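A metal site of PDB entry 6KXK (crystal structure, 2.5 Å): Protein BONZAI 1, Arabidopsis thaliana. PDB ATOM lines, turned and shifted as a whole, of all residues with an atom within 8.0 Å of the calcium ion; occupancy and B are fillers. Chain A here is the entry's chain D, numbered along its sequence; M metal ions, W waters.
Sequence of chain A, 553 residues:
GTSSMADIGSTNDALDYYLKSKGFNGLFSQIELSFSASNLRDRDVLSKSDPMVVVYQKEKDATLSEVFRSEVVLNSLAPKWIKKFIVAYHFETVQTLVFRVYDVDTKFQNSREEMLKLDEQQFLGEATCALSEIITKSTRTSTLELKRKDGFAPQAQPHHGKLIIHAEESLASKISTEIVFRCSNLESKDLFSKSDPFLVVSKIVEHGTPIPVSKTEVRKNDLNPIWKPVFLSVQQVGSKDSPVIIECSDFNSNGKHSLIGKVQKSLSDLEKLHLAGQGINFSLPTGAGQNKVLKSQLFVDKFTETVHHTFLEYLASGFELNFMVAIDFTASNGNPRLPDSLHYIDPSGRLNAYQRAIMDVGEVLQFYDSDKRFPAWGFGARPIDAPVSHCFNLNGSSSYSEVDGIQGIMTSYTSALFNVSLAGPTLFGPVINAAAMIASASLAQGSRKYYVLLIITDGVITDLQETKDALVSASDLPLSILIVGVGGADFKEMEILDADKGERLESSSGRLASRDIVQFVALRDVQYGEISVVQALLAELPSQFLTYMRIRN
Merely in contact with the calcium ion: Glu 402 (3.7 Å). Of the 18 residues printed, 4 come within 4 Å of the calcium ion. The nearest printed residue that does not touch the calcium ion is Asn 322 (4.2 Å).
ND2 of Asn 322 sits close to OD2 of Asp 369, at 3.1 Å. The backbone carbonyl oxygen (O) of Asp 369 sits at hydrogen-bond distance from the side-chain amino group (NZ) of Lys 372 (2.8 Å). The side-chain hydroxyl (OH) of Tyr 400 sits at hydrogen-bond distance from the side-chain carboxylate (OE2) of Glu 402, at 2.8 Å.
The calcium ion is bound by water W1 (2.2 Å), the side-chain carboxylate (OD1) of Asp 371 (2.3 Å), the backbone carbonyl oxygen (O) of Arg 373 (2.3 Å), the side-chain carboxylate (OD2) of Asp 369 (2.4 Å) and the side-chain carboxylate (OD1) of Asp 369 (2.9 Å). The calcium ion has five donor atoms within binding distance.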
ATOM      1  N   GLU A 320      22.687 -32.166  24.411  1.00  0.00           N
ATOM      2  CA  GLU A 320      22.651 -30.873  25.037  1.00  0.00           C
ATOM      3  C   GLU A 320      22.388 -31.008  26.524  1.00  0.00           C
ATOM      4  O   GLU A 320      21.780 -31.978  26.964  1.00  0.00           O
ATOM      5  CB  GLU A 320      21.533 -30.045  24.420  1.00  0.00           C
ATOM      6  CG  GLU A 320      21.741 -29.621  23.003  1.00  0.00           C
ATOM      7  CD  GLU A 320      20.486 -28.854  22.539  1.00  0.00           C
ATOM      8  OE1 GLU A 320      20.319 -27.652  22.937  1.00  0.00           O
ATOM      9  OE2 GLU A 320      19.676 -29.403  21.716  1.00  0.00           O
ATOM     10  N   LEU A 321      22.865 -30.008  27.263  1.00  0.00           N
ATOM     11  CA  LEU A 321      22.383 -29.777  28.602  1.00  0.00           C
ATOM     12  C   LEU A 321      21.504 -28.537  28.569  1.00  0.00           C
ATOM     13  O   LEU A 321      21.946 -27.467  28.170  1.00  0.00           O
ATOM     14  CB  LEU A 321      23.577 -29.603  29.528  1.00  0.00           C
ATOM     15  CG  LEU A 321      24.479 -30.835  29.671  1.00  0.00           C
ATOM     16  CD1 LEU A 321      25.600 -30.622  30.617  1.00  0.00           C
ATOM     17  CD2 LEU A 321      23.691 -31.984  30.229  1.00  0.00           C
ATOM     18  N   ASN A 322      20.250 -28.688  28.984  1.00  0.00           N
ATOM     19  CA  ASN A 322      19.219 -27.656  28.865  1.00  0.00           C
ATOM     20  C   ASN A 322      18.849 -27.142  30.247  1.00  0.00           C
ATOM     21  O   ASN A 322      18.199 -27.859  31.014  1.00  0.00           O
ATOM     22  CB  ASN A 322      18.037 -28.135  27.997  1.00  0.00           C
ATOM     23  CG  ASN A 322      18.587 -28.913  26.825  1.00  0.00           C
ATOM     24  OD1 ASN A 322      19.042 -30.044  26.965  1.00  0.00           O
ATOM     25  ND2 ASN A 322      18.646 -28.283  25.679  1.00  0.00           N
ATOM     26  N   PHE A 323      19.227 -25.869  30.515  1.00  0.00           N
ATOM     27  CA  PHE A 323      19.101 -25.257  31.821  1.00  0.00           C
ATOM     28  C   PHE A 323      17.641 -24.864  32.035  1.00  0.00           C
ATOM     29  O   PHE A 323      16.982 -24.367  31.128  1.00  0.00           O
ATOM     30  CB  PHE A 323      19.977 -24.022  31.864  1.00  0.00           C
ATOM     31  CG  PHE A 323      19.936 -23.152  33.090  1.00  0.00           C
ATOM     32  CD1 PHE A 323      19.922 -23.712  34.352  1.00  0.00           C
ATOM     33  CD2 PHE A 323      19.955 -21.759  32.961  1.00  0.00           C
ATOM     34  CE1 PHE A 323      19.902 -22.876  35.470  1.00  0.00           C
ATOM     35  CE2 PHE A 323      19.966 -20.932  34.072  1.00  0.00           C
ATOM     36  CZ  PHE A 323      19.953 -21.502  35.325  1.00  0.00           C
ATOM     37  N   GLN A 366      24.587 -22.143  29.768  1.00  0.00           N
ATOM     38  CA  GLN A 366      24.002 -21.568  28.568  1.00  0.00           C
ATOM     39  C   GLN A 366      24.655 -22.111  27.301  1.00  0.00           C
ATOM     40  O   GLN A 366      23.986 -22.289  26.283  1.00  0.00           O
ATOM     41  CB  GLN A 366      24.029 -20.031  28.536  1.00  0.00           C
ATOM     42  CG  GLN A 366      25.377 -19.436  28.300  1.00  0.00           C
ATOM     43  CD  GLN A 366      25.458 -17.945  28.583  1.00  0.00           C
ATOM     44  OE1 GLN A 366      24.570 -17.177  28.201  1.00  0.00           O
ATOM     45  NE2 GLN A 366      26.520 -17.510  29.276  1.00  0.00           N
ATOM     46  N   TYR A 368      25.643 -24.985  26.489  1.00  0.00           N
ATOM     47  CA  TYR A 368      25.348 -26.372  26.185  1.00  0.00           C
ATOM     48  C   TYR A 368      23.932 -26.553  25.617  1.00  0.00           C
ATOM     49  O   TYR A 368      23.517 -27.665  25.326  1.00  0.00           O
ATOM     50  CB  TYR A 368      25.652 -27.263  27.392  1.00  0.00           C
ATOM     51  CG  TYR A 368      27.090 -27.170  27.817  1.00  0.00           C
ATOM     52  CD1 TYR A 368      27.517 -26.218  28.727  1.00  0.00           C
ATOM     53  CD2 TYR A 368      28.036 -28.010  27.275  1.00  0.00           C
ATOM     54  CE1 TYR A 368      28.847 -26.111  29.094  1.00  0.00           C
ATOM     55  CE2 TYR A 368      29.378 -27.914  27.614  1.00  0.00           C
ATOM     56  CZ  TYR A 368      29.779 -26.950  28.517  1.00  0.00           C
ATOM     57  OH  TYR A 368      31.083 -26.840  28.869  1.00  0.00           O
ATOM     58  N   ASP A 369      23.199 -25.427  25.440  1.00  0.00           N
ATOM     59  CA  ASP A 369      21.881 -25.382  24.828  1.00  0.00           C
ATOM     60  C   ASP A 369      21.983 -24.586  23.520  1.00  0.00           C
ATOM     61  O   ASP A 369      22.643 -23.523  23.464  1.00  0.00           O
ATOM     62  CB  ASP A 369      20.912 -24.750  25.819  1.00  0.00           C
ATOM     63  CG  ASP A 369      19.439 -24.465  25.453  1.00  0.00           C
ATOM     64  OD1 ASP A 369      19.142 -23.433  24.802  1.00  0.00           O
ATOM     65  OD2 ASP A 369      18.525 -25.170  25.969  1.00  0.00           O
ATOM     66  N   SER A 370      21.404 -25.173  22.463  1.00  0.00           N
ATOM     67  CA  SER A 370      21.730 -24.743  21.104  1.00  0.00           C
ATOM     68  C   SER A 370      20.834 -23.588  20.639  1.00  0.00           C
ATOM     69  O   SER A 370      21.294 -22.667  19.975  1.00  0.00           O
ATOM     70  CB  SER A 370      21.680 -25.856  20.129  1.00  0.00           C
ATOM     71  OG  SER A 370      20.472 -26.587  20.329  1.00  0.00           O
ATOM     72  N   ASP A 371      19.545 -23.647  21.025  1.00  0.00           N
ATOM     73  CA  ASP A 371      18.607 -22.573  20.726  1.00  0.00           C
ATOM     74  C   ASP A 371      18.780 -21.415  21.708  1.00  0.00           C
ATOM     75  O   ASP A 371      18.364 -20.330  21.372  1.00  0.00           O
ATOM     76  CB  ASP A 371      17.190 -23.067  20.492  1.00  0.00           C
ATOM     77  CG  ASP A 371      16.495 -23.501  21.752  1.00  0.00           C
ATOM     78  OD1 ASP A 371      17.044 -23.372  22.870  1.00  0.00           O
ATOM     79  OD2 ASP A 371      15.355 -23.892  21.616  1.00  0.00           O
ATOM     80  N   LYS A 372      19.281 -21.647  22.927  1.00  0.00           N
ATOM     81  CA  LYS A 372      19.420 -20.638  23.971  1.00  0.00           C
ATOM     82  C   LYS A 372      18.041 -20.127  24.370  1.00  0.00           C
ATOM     83  O   LYS A 372      17.817 -18.934  24.532  1.00  0.00           O
ATOM     84  CB  LYS A 372      20.463 -19.571  23.590  1.00  0.00           C
ATOM     85  CG  LYS A 372      21.817 -20.180  23.252  1.00  0.00           C
ATOM     86  CD  LYS A 372      23.047 -19.400  23.646  1.00  0.00           C
ATOM     87  CE  LYS A 372      24.264 -20.062  23.048  1.00  0.00           C
ATOM     88  NZ  LYS A 372      24.451 -21.423  23.601  1.00  0.00           N
ATOM     89  N   ARG A 373      17.099 -21.065  24.479  1.00  0.00           N
ATOM     90  CA  ARG A 373      15.760 -20.843  24.995  1.00  0.00           C
ATOM     91  C   ARG A 373      15.640 -21.842  26.144  1.00  0.00           C
ATOM     92  O   ARG A 373      15.741 -23.039  25.899  1.00  0.00           O
ATOM     93  CB  ARG A 373      14.678 -21.164  23.938  1.00  0.00           C
ATOM     94  CG  ARG A 373      14.783 -20.473  22.576  1.00  0.00           C
ATOM     95  CD  ARG A 373      13.427 -20.464  21.988  1.00  0.00           C
ATOM     96  NE  ARG A 373      12.818 -19.150  22.196  1.00  0.00           N
ATOM     97  CZ  ARG A 373      11.524 -18.941  22.419  1.00  0.00           C
ATOM     98  NH1 ARG A 373      11.088 -17.700  22.579  1.00  0.00           N
ATOM     99  NH2 ARG A 373      10.656 -19.943  22.470  1.00  0.00           N
ATOM    100  N   PHE A 374      15.195 -21.348  27.341  1.00  0.00           N
ATOM    101  CA  PHE A 374      15.213 -21.939  28.662  1.00  0.00           C
ATOM    102  C   PHE A 374      13.849 -21.818  29.376  1.00  0.00           C
ATOM    103  O   PHE A 374      13.309 -20.725  29.527  1.00  0.00           O
ATOM    104  CB  PHE A 374      16.221 -21.133  29.512  1.00  0.00           C
ATOM    105  CG  PHE A 374      17.614 -21.107  28.987  1.00  0.00           C
ATOM    106  CD1 PHE A 374      18.360 -22.286  28.972  1.00  0.00           C
ATOM    107  CD2 PHE A 374      18.195 -19.919  28.487  1.00  0.00           C
ATOM    108  CE1 PHE A 374      19.660 -22.251  28.478  1.00  0.00           C
ATOM    109  CE2 PHE A 374      19.473 -19.903  28.011  1.00  0.00           C
ATOM    110  CZ  PHE A 374      20.131 -21.108  27.868  1.00  0.00           C
ATOM    111  N   PRO A 375      13.315 -22.920  29.935  1.00  0.00           N
ATOM    112  CA  PRO A 375      12.163 -22.824  30.825  1.00  0.00           C
ATOM    113  C   PRO A 375      12.555 -22.045  32.082  1.00  0.00           C
ATOM    114  O   PRO A 375      13.544 -22.389  32.748  1.00  0.00           O
ATOM    115  CB  PRO A 375      11.845 -24.276  31.211  1.00  0.00           C
ATOM    116  CG  PRO A 375      12.558 -25.126  30.165  1.00  0.00           C
ATOM    117  CD  PRO A 375      13.724 -24.305  29.656  1.00  0.00           C
ATOM    118  N   TYR A 400       3.166 -23.831  27.836  1.00  0.00           N
ATOM    119  CA  TYR A 400       4.616 -23.956  27.894  1.00  0.00           C
ATOM    120  C   TYR A 400       5.333 -22.796  27.190  1.00  0.00           C
ATOM    121  O   TYR A 400       4.907 -22.325  26.129  1.00  0.00           O
ATOM    122  CB  TYR A 400       5.038 -25.298  27.300  1.00  0.00           C
ATOM    123  CG  TYR A 400       6.497 -25.573  27.457  1.00  0.00           C
ATOM    124  CD1 TYR A 400       6.967 -26.072  28.658  1.00  0.00           C
ATOM    125  CD2 TYR A 400       7.411 -25.298  26.445  1.00  0.00           C
ATOM    126  CE1 TYR A 400       8.323 -26.327  28.845  1.00  0.00           C
ATOM    127  CE2 TYR A 400       8.767 -25.523  26.631  1.00  0.00           C
ATOM    128  CZ  TYR A 400       9.211 -26.070  27.828  1.00  0.00           C
ATOM    129  OH  TYR A 400      10.543 -26.319  28.015  1.00  0.00           O
ATOM    130  N   GLU A 402       9.493 -21.186  26.714  1.00  0.00           N
ATOM    131  CA  GLU A 402      10.894 -20.914  27.006  1.00  0.00           C
ATOM    132  C   GLU A 402      11.107 -19.392  26.959  1.00  0.00           C
ATOM    133  O   GLU A 402      10.463 -18.731  26.179  1.00  0.00           O
ATOM    134  CB  GLU A 402      11.732 -21.731  26.011  1.00  0.00           C
ATOM    135  CG  GLU A 402      11.769 -23.196  26.472  1.00  0.00           C
ATOM    136  CD  GLU A 402      12.168 -24.277  25.493  1.00  0.00           C
ATOM    137  OE1 GLU A 402      12.966 -23.977  24.576  1.00  0.00           O
ATOM    138  OE2 GLU A 402      11.695 -25.417  25.673  1.00  0.00           O
ATOM    139  N   VAL A 403      12.160 -18.873  27.592  1.00  0.00           N
ATOM    140  CA  VAL A 403      12.585 -17.482  27.459  1.00  0.00           C
ATOM    141  C   VAL A 403      13.928 -17.413  26.727  1.00  0.00           C
ATOM    142  O   VAL A 403      14.657 -18.381  26.670  1.00  0.00           O
ATOM    143  CB  VAL A 403      12.613 -16.767  28.827  1.00  0.00           C
ATOM    144  CG1 VAL A 403      11.332 -16.970  29.596  1.00  0.00           C
ATOM    145  CG2 VAL A 403      13.792 -17.216  29.689  1.00  0.00           C
ATOM    146  N   LYS A 449      18.170 -33.985  24.531  1.00  0.00           N
ATOM    147  CA  LYS A 449      18.277 -33.016  25.593  1.00  0.00           C
ATOM    148  C   LYS A 449      18.367 -33.721  26.951  1.00  0.00           C
ATOM    149  O   LYS A 449      17.749 -34.748  27.191  1.00  0.00           O
ATOM    150  CB  LYS A 449      17.082 -32.050  25.547  1.00  0.00           C
ATOM    151  CG  LYS A 449      17.061 -31.088  24.379  1.00  0.00           C
ATOM    152  CD  LYS A 449      15.847 -30.211  24.498  1.00  0.00           C
ATOM    153  CE  LYS A 449      15.605 -29.281  23.330  1.00  0.00           C
ATOM    154  NZ  LYS A 449      14.439 -28.424  23.622  1.00  0.00           N
ATOM    155  N   TYR A 451      18.097 -32.313  30.908  1.00  0.00           N
ATOM    156  CA  TYR A 451      17.677 -31.117  31.607  1.00  0.00           C
ATOM    157  C   TYR A 451      18.414 -30.963  32.927  1.00  0.00           C
ATOM    158  O   TYR A 451      18.656 -31.955  33.622  1.00  0.00           O
ATOM    159  CB  TYR A 451      16.151 -31.053  31.761  1.00  0.00           C
ATOM    160  CG  TYR A 451      15.434 -30.870  30.456  1.00  0.00           C
ATOM    161  CD1 TYR A 451      15.298 -29.613  29.874  1.00  0.00           C
ATOM    162  CD2 TYR A 451      15.017 -31.979  29.737  1.00  0.00           C
ATOM    163  CE1 TYR A 451      14.610 -29.446  28.683  1.00  0.00           C
ATOM    164  CE2 TYR A 451      14.394 -31.832  28.502  1.00  0.00           C
ATOM    165  CZ  TYR A 451      14.186 -30.571  27.980  1.00  0.00           C
ATOM    166  OH  TYR A 451      13.598 -30.437  26.763  1.00  0.00           O
HETATM  167 CA    CA M   1      16.625 -24.772  24.612  1.00  0.00          CA
HETATM  168  O   HOH W   1      15.623 -26.094  26.060  1.00  0.00           O
